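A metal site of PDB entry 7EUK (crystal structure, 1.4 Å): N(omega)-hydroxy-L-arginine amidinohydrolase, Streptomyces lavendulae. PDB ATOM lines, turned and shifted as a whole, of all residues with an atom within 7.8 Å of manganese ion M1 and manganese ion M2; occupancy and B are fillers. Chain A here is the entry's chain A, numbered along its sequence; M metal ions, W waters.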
ATOM      1  N   THR A  85      30.969  -0.742  34.765  1.00  0.00           N
ATOM      2  CA  THR A  85      30.409  -1.870  34.016  1.00  0.00           C
ATOM      3  C   THR A  85      29.549  -1.364  32.867  1.00  0.00           C
ATOM      4  O   THR A  85      29.084  -0.216  32.876  1.00  0.00           O
ATOM      5  CB  THR A  85      29.543  -2.775  34.895  1.00  0.00           C
ATOM      6  OG1 THR A  85      28.439  -2.016  35.404  1.00  0.00           O
ATOM      7  CG2 THR A  85      30.333  -3.361  36.062  1.00  0.00           C
ATOM      8  N   CYS A  86      29.354  -2.226  31.870  1.00  0.00           N
ATOM      9  CA  CYS A  86      28.431  -1.892  30.796  1.00  0.00           C
ATOM     10  C   CYS A  86      27.040  -1.613  31.314  1.00  0.00           C
ATOM     11  O   CYS A  86      26.301  -0.856  30.673  1.00  0.00           O
ATOM     12  CB  CYS A  86      28.380  -3.010  29.760  1.00  0.00           C
ATOM     13  SG  CYS A  86      29.845  -3.146  28.718  1.00  0.00           S
ATOM     14  N   SER A  87      26.671  -2.214  32.456  1.00  0.00           N
ATOM     15  CA  SER A  87      25.302  -2.066  32.959  1.00  0.00           C
ATOM     16  C   SER A  87      24.948  -0.637  33.334  1.00  0.00           C
ATOM     17  O   SER A  87      23.749  -0.308  33.389  1.00  0.00           O
ATOM     18  CB  SER A  87      25.072  -2.963  34.176  1.00  0.00           C
ATOM     19  OG  SER A  87      25.195  -4.325  33.823  1.00  0.00           O
ATOM     20  N   TYR A 107      27.999  -0.203  19.748  1.00  0.00           N
ATOM     21  CA  TYR A 107      28.180  -0.959  20.988  1.00  0.00           C
ATOM     22  C   TYR A 107      29.363  -1.882  20.739  1.00  0.00           C
ATOM     23  O   TYR A 107      29.231  -2.947  20.112  1.00  0.00           O
ATOM     24  CB  TYR A 107      26.893  -1.693  21.338  1.00  0.00           C
ATOM     25  CG  TYR A 107      26.794  -2.123  22.793  1.00  0.00           C
ATOM     26  CD1 TYR A 107      27.447  -3.273  23.235  1.00  0.00           C
ATOM     27  CD2 TYR A 107      26.051  -1.407  23.723  1.00  0.00           C
ATOM     28  CE1 TYR A 107      27.374  -3.678  24.555  1.00  0.00           C
ATOM     29  CE2 TYR A 107      25.956  -1.807  25.041  1.00  0.00           C
ATOM     30  CZ  TYR A 107      26.627  -2.953  25.450  1.00  0.00           C
ATOM     31  OH  TYR A 107      26.546  -3.370  26.771  1.00  0.00           O
ATOM     32  N   ILE A 108      30.532  -1.438  21.167  1.00  0.00           N
ATOM     33  CA  ILE A 108      31.806  -2.065  20.839  1.00  0.00           C
ATOM     34  C   ILE A 108      32.156  -2.997  21.996  1.00  0.00           C
ATOM     35  O   ILE A 108      32.471  -2.551  23.092  1.00  0.00           O
ATOM     36  CB  ILE A 108      32.895  -1.013  20.582  1.00  0.00           C
ATOM     37  CG1 ILE A 108      32.397   0.028  19.563  1.00  0.00           C
ATOM     38  CG2 ILE A 108      34.188  -1.695  20.099  1.00  0.00           C
ATOM     39  CD1 ILE A 108      33.450   1.060  19.181  1.00  0.00           C
ATOM     40  N   ASP A 109      32.104  -4.302  21.755  1.00  0.00           N
ATOM     41  CA  ASP A 109      32.106  -5.275  22.845  1.00  0.00           C
ATOM     42  C   ASP A 109      32.443  -6.633  22.253  1.00  0.00           C
ATOM     43  O   ASP A 109      31.987  -6.952  21.149  1.00  0.00           O
ATOM     44  CB  ASP A 109      30.685  -5.292  23.486  1.00  0.00           C
ATOM     45  CG  ASP A 109      30.662  -5.898  24.874  1.00  0.00           C
ATOM     46  OD1 ASP A 109      31.326  -6.936  25.103  1.00  0.00           O
ATOM     47  OD2 ASP A 109      29.971  -5.333  25.765  1.00  0.00           O
ATOM     48  N   GLY A 110      33.243  -7.439  22.963  1.00  0.00           N
ATOM     49  CA  GLY A 110      33.459  -8.798  22.502  1.00  0.00           C
ATOM     50  C   GLY A 110      32.224  -9.671  22.618  1.00  0.00           C
ATOM     51  O   GLY A 110      32.167 -10.749  21.987  1.00  0.00           O
ATOM     52  N   HIS A 111      31.243  -9.233  23.409  1.00  0.00           N
ATOM     53  CA  HIS A 111      29.977  -9.923  23.611  1.00  0.00           C
ATOM     54  C   HIS A 111      28.851  -9.155  22.953  1.00  0.00           C
ATOM     55  O   HIS A 111      28.997  -7.983  22.579  1.00  0.00           O
ATOM     56  CB  HIS A 111      29.643  -9.991  25.106  1.00  0.00           C
ATOM     57  CG  HIS A 111      30.663 -10.709  25.917  1.00  0.00           C
ATOM     58  ND1 HIS A 111      31.735 -10.063  26.500  1.00  0.00           N
ATOM     59  CD2 HIS A 111      30.788 -12.015  26.261  1.00  0.00           C
ATOM     60  CE1 HIS A 111      32.468 -10.939  27.170  1.00  0.00           C
ATOM     61  NE2 HIS A 111      31.913 -12.127  27.042  1.00  0.00           N
ATOM     62  N   GLY A 112      27.687  -9.813  22.843  1.00  0.00           N
ATOM     63  CA  GLY A 112      26.507  -9.125  22.344  1.00  0.00           C
ATOM     64  C   GLY A 112      25.734  -8.340  23.397  1.00  0.00           C
ATOM     65  O   GLY A 112      25.004  -7.412  23.051  1.00  0.00           O
ATOM     66  N   ASP A 113      25.877  -8.714  24.682  1.00  0.00           N
ATOM     67  CA  ASP A 113      25.137  -8.088  25.780  1.00  0.00           C
ATOM     68  C   ASP A 113      23.651  -7.966  25.456  1.00  0.00           C
ATOM     69  O   ASP A 113      23.014  -6.958  25.772  1.00  0.00           O
ATOM     70  CB  ASP A 113      25.749  -6.734  26.169  1.00  0.00           C
ATOM     71  CG  ASP A 113      27.104  -6.870  26.829  1.00  0.00           C
ATOM     72  OD1 ASP A 113      27.637  -8.002  26.936  1.00  0.00           O
ATOM     73  OD2 ASP A 113      27.631  -5.833  27.279  1.00  0.00           O
ATOM     74  N   TYR A 124      23.682 -12.608  34.762  1.00  0.00           N
ATOM     75  CA  TYR A 124      24.494 -11.409  34.917  1.00  0.00           C
ATOM     76  C   TYR A 124      23.875 -10.218  34.164  1.00  0.00           C
ATOM     77  O   TYR A 124      23.661 -10.278  32.949  1.00  0.00           O
ATOM     78  CB  TYR A 124      25.924 -11.684  34.440  1.00  0.00           C
ATOM     79  CG  TYR A 124      26.837 -10.487  34.484  1.00  0.00           C
ATOM     80  CD1 TYR A 124      26.879  -9.650  35.595  1.00  0.00           C
ATOM     81  CD2 TYR A 124      27.646 -10.200  33.403  1.00  0.00           C
ATOM     82  CE1 TYR A 124      27.727  -8.547  35.617  1.00  0.00           C
ATOM     83  CE2 TYR A 124      28.477  -9.097  33.408  1.00  0.00           C
ATOM     84  CZ  TYR A 124      28.527  -8.265  34.517  1.00  0.00           C
ATOM     85  OH  TYR A 124      29.368  -7.170  34.489  1.00  0.00           O
ATOM     86  N   GLY A 126      25.169  -7.492  33.273  1.00  0.00           N
ATOM     87  CA  GLY A 126      26.045  -6.951  32.247  1.00  0.00           C
ATOM     88  C   GLY A 126      25.906  -7.646  30.908  1.00  0.00           C
ATOM     89  O   GLY A 126      26.342  -7.093  29.892  1.00  0.00           O
ATOM     90  N   GLY A 127      25.317  -8.833  30.868  1.00  0.00           N
ATOM     91  CA  GLY A 127      25.026  -9.496  29.611  1.00  0.00           C
ATOM     92  C   GLY A 127      23.670  -9.170  29.039  1.00  0.00           C
ATOM     93  O   GLY A 127      23.275  -9.793  28.050  1.00  0.00           O
ATOM     94  N   MET A 128      22.967  -8.195  29.623  1.00  0.00           N
ATOM     95  CA  MET A 128      21.585  -7.880  29.282  1.00  0.00           C
ATOM     96  C   MET A 128      21.401  -6.403  28.951  1.00  0.00           C
ATOM     97  O   MET A 128      20.267  -5.921  28.899  1.00  0.00           O
ATOM     98  CB  MET A 128      20.658  -8.246  30.464  1.00  0.00           C
ATOM     99  CG  MET A 128      20.777  -9.698  30.936  1.00  0.00           C
ATOM    100  SD  MET A 128      20.131 -10.079  32.583  1.00  0.00           S
ATOM    101  CE  MET A 128      18.396  -9.767  32.333  1.00  0.00           C
ATOM    102  N   VAL A 129      22.497  -5.678  28.718  1.00  0.00           N
ATOM    103  CA  VAL A 129      22.448  -4.217  28.645  1.00  0.00           C
ATOM    104  C   VAL A 129      21.799  -3.741  27.363  1.00  0.00           C
ATOM    105  O   VAL A 129      20.887  -2.901  27.382  1.00  0.00           O
ATOM    106  CB  VAL A 129      23.865  -3.644  28.806  1.00  0.00           C
ATOM    107  CG1 VAL A 129      23.848  -2.124  28.671  1.00  0.00           C
ATOM    108  CG2 VAL A 129      24.469  -4.057  30.132  1.00  0.00           C
ATOM    109  N   LEU A 130      22.284  -4.207  26.214  1.00  0.00           N
ATOM    110  CA  LEU A 130      21.788  -3.674  24.959  1.00  0.00           C
ATOM    111  C   LEU A 130      20.348  -4.096  24.721  1.00  0.00           C
ATOM    112  O   LEU A 130      19.530  -3.305  24.240  1.00  0.00           O
ATOM    113  CB  LEU A 130      22.709  -4.065  23.808  1.00  0.00           C
ATOM    114  CG  LEU A 130      22.382  -3.528  22.411  1.00  0.00           C
ATOM    115  CD1 LEU A 130      22.366  -2.011  22.371  1.00  0.00           C
ATOM    116  CD2 LEU A 130      23.381  -4.081  21.425  1.00  0.00           C
ATOM    117  N   SER A 155      31.997  -7.987  18.225  1.00  0.00           N
ATOM    118  CA  SER A 155      31.428  -9.127  18.921  1.00  0.00           C
ATOM    119  C   SER A 155      31.715 -10.402  18.142  1.00  0.00           C
ATOM    120  O   SER A 155      31.748 -10.413  16.917  1.00  0.00           O
ATOM    121  CB  SER A 155      29.916  -8.944  19.016  1.00  0.00           C
ATOM    122  OG  SER A 155      29.588  -7.664  19.512  1.00  0.00           O
ATOM    123  N   HIS A 196      29.889   3.237  22.735  1.00  0.00           N
ATOM    124  CA  HIS A 196      29.980   2.520  23.999  1.00  0.00           C
ATOM    125  C   HIS A 196      31.031   1.426  23.834  1.00  0.00           C
ATOM    126  O   HIS A 196      30.914   0.582  22.944  1.00  0.00           O
ATOM    127  CB  HIS A 196      28.618   1.886  24.294  1.00  0.00           C
ATOM    128  CG  HIS A 196      28.619   0.908  25.436  1.00  0.00           C
ATOM    129  ND1 HIS A 196      27.991   1.183  26.633  1.00  0.00           N
ATOM    130  CD2 HIS A 196      29.166  -0.323  25.554  1.00  0.00           C
ATOM    131  CE1 HIS A 196      28.157   0.149  27.454  1.00  0.00           C
ATOM    132  NE2 HIS A 196      28.879  -0.775  26.826  1.00  0.00           N
ATOM    133  N   ILE A 197      32.066   1.432  24.682  1.00  0.00           N
ATOM    134  CA  ILE A 197      33.147   0.432  24.582  1.00  0.00           C
ATOM    135  C   ILE A 197      33.244  -0.395  25.858  1.00  0.00           C
ATOM    136  O   ILE A 197      33.350   0.163  26.955  1.00  0.00           O
ATOM    137  CB  ILE A 197      34.505   1.067  24.273  1.00  0.00           C
ATOM    138  CG1 ILE A 197      34.473   1.776  22.936  1.00  0.00           C
ATOM    139  CG2 ILE A 197      35.590  -0.013  24.239  1.00  0.00           C
ATOM    140  CD1 ILE A 197      35.684   2.691  22.727  1.00  0.00           C
ATOM    141  N   ASP A 198      33.235  -1.728  25.700  1.00  0.00           N
ATOM    142  CA  ASP A 198      33.643  -2.698  26.716  1.00  0.00           C
ATOM    143  C   ASP A 198      35.025  -3.189  26.293  1.00  0.00           C
ATOM    144  O   ASP A 198      35.181  -3.764  25.214  1.00  0.00           O
ATOM    145  CB  ASP A 198      32.612  -3.821  26.692  1.00  0.00           C
ATOM    146  CG  ASP A 198      32.919  -5.008  27.621  1.00  0.00           C
ATOM    147  OD1 ASP A 198      34.062  -5.136  28.077  1.00  0.00           O
ATOM    148  OD2 ASP A 198      31.980  -5.839  27.830  1.00  0.00           O
ATOM    149  N   TRP A 199      36.030  -2.965  27.151  1.00  0.00           N
ATOM    150  CA  TRP A 199      37.407  -3.285  26.757  1.00  0.00           C
ATOM    151  C   TRP A 199      37.649  -4.763  26.484  1.00  0.00           C
ATOM    152  O   TRP A 199      38.694  -5.076  25.892  1.00  0.00           O
ATOM    153  CB  TRP A 199      38.445  -2.755  27.776  1.00  0.00           C
ATOM    154  CG  TRP A 199      38.376  -1.267  27.914  1.00  0.00           C
ATOM    155  CD1 TRP A 199      38.087  -0.565  29.056  1.00  0.00           C
ATOM    156  CD2 TRP A 199      38.599  -0.295  26.886  1.00  0.00           C
ATOM    157  NE1 TRP A 199      38.105   0.776  28.798  1.00  0.00           N
ATOM    158  CE2 TRP A 199      38.409   0.973  27.466  1.00  0.00           C
ATOM    159  CE3 TRP A 199      38.919  -0.367  25.523  1.00  0.00           C
ATOM    160  CZ2 TRP A 199      38.541   2.164  26.747  1.00  0.00           C
ATOM    161  CZ3 TRP A 199      39.035   0.817  24.806  1.00  0.00           C
ATOM    162  CH2 TRP A 199      38.850   2.059  25.419  1.00  0.00           C
ATOM    163  N   ASP A 200      36.731  -5.662  26.872  1.00  0.00           N
ATOM    164  CA  ASP A 200      36.935  -7.050  26.477  1.00  0.00           C
ATOM    165  C   ASP A 200      36.824  -7.275  24.963  1.00  0.00           C
ATOM    166  O   ASP A 200      37.097  -8.380  24.485  1.00  0.00           O
ATOM    167  CB  ASP A 200      36.090  -8.047  27.293  1.00  0.00           C
ATOM    168  CG  ASP A 200      34.601  -7.935  27.027  1.00  0.00           C
ATOM    169  OD1 ASP A 200      34.166  -7.545  25.921  1.00  0.00           O
ATOM    170  OD2 ASP A 200      33.818  -8.282  27.951  1.00  0.00           O
ATOM    171  N   VAL A 201      36.480  -6.238  24.192  1.00  0.00           N
ATOM    172  CA  VAL A 201      36.539  -6.373  22.739  1.00  0.00           C
ATOM    173  C   VAL A 201      37.971  -6.542  22.248  1.00  0.00           C
ATOM    174  O   VAL A 201      38.188  -7.114  21.162  1.00  0.00           O
ATOM    175  CB  VAL A 201      35.860  -5.147  22.083  1.00  0.00           C
ATOM    176  CG1 VAL A 201      36.748  -3.908  22.157  1.00  0.00           C
ATOM    177  CG2 VAL A 201      35.480  -5.461  20.633  1.00  0.00           C
ATOM    178  N   ALA A 240      34.059   1.453  29.363  1.00  0.00           N
ATOM    179  CA  ALA A 240      33.606   0.547  30.414  1.00  0.00           C
ATOM    180  C   ALA A 240      34.465  -0.708  30.530  1.00  0.00           C
ATOM    181  O   ALA A 240      35.040  -1.184  29.548  1.00  0.00           O
ATOM    182  CB  ALA A 240      32.152   0.125  30.172  1.00  0.00           C
ATOM    183  N   GLU A 241      34.538  -1.226  31.762  1.00  0.00           N
ATOM    184  CA  GLU A 241      35.044  -2.578  32.048  1.00  0.00           C
ATOM    185  C   GLU A 241      36.560  -2.712  31.861  1.00  0.00           C
ATOM    186  O   GLU A 241      37.047  -3.673  31.257  1.00  0.00           O
ATOM    187  CB  GLU A 241      34.248  -3.668  31.323  1.00  0.00           C
ATOM    188  CG  GLU A 241      32.760  -3.478  31.485  1.00  0.00           C
ATOM    189  CD  GLU A 241      31.972  -4.762  31.646  1.00  0.00           C
ATOM    190  OE1 GLU A 241      32.536  -5.874  31.478  1.00  0.00           O
ATOM    191  OE2 GLU A 241      30.741  -4.666  31.894  1.00  0.00           O
HETATM  192 MN    MN M   1      31.992  -7.837  26.873  1.00  0.00          MN
HETATM  193 MN    MN M   2      29.759  -5.491  27.887  1.00  0.00          MN
HETATM  194  O   HOH W   1      30.017  -7.847  27.900  1.00  0.00           O
HETATM  195  O   HOH W   2      29.344  -6.111  29.935  1.00  0.00           O
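The backbone NH (N) of Asp 198 lies within hydrogen-bond range of the backbone carbonyl oxygen (O) of Ile 108, at 2.8 Å. OD1 of Asp 200 sits close to N of Gly 110 (3.1 Å). The backbone NH of Val 129 sits at hydrogen-bond distance from the backbone carbonyl oxygen of Asp 113, 3.3 Å away. The side-chain sulfur of Cys 86 sits close to a ring nitrogen (NE2) of His 196. The backbone NH (N) of Cys 86 sits at hydrogen-bond distance from the side-chain carboxylate (OE2) of Glu 241, 2.8 Å away. The backbone carbonyl oxygen (O) of Asp 113 is in hydrogen-bond range of the backbone NH (N) of Leu 130 (2.9 Å). The backbone carbonyl oxygen (O) of Asp 109 lies within hydrogen-bond range of the side-chain hydroxyl (OG) of Ser 155, at 3.0 Å. The side-chain hydroxyl (OH) of Tyr 107 lies close to the side-chain carboxylate (OD2) of Asp 113 (2.7 Å).
The nearest printed residue that does not touch manganese ion M1 is Gly 110 (4.1 Å).
Four residues have an atom within 4 Å of manganese ion M2: Cys 86, Asp 109, Asp 113 and Asp 198. Along chain A the residues within 4 Å of manganese ion M2 span positions 86 to 198. The nearest printed residue that does not touch manganese ion M2 is Tyr 107 (4.01 Å).
Manganese ion M1 is bound by OD1 of Asp 109, OD2 of Asp 200, OD2 of Asp 198, water W1, ND1 of His 111 and OD1 of Asp 200. Manganese ion M1 has six donor atoms within binding distance.
OD2 of Asp 109 binds manganese ion M2. Water W2 is bound to manganese ion M2, 2.2 Å away. The side-chain carboxylate (OD2) of Asp 113 binds manganese ion M2, 2.2 Å away. OD2 of Asp 198 is bound to manganese ion M2 (2.2 Å). Manganese ion M2 is bound by water W1 (2.4 Å). SG of Cys 86 is bound to manganese ion M2, at 2.5 Å. Manganese ion M2 has six donor atoms within binding distance.
Water W2 lies within hydrogen-bond range of OE2 of Glu 241 (2.8 Å) and O of Gly 126 (3.2 Å).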
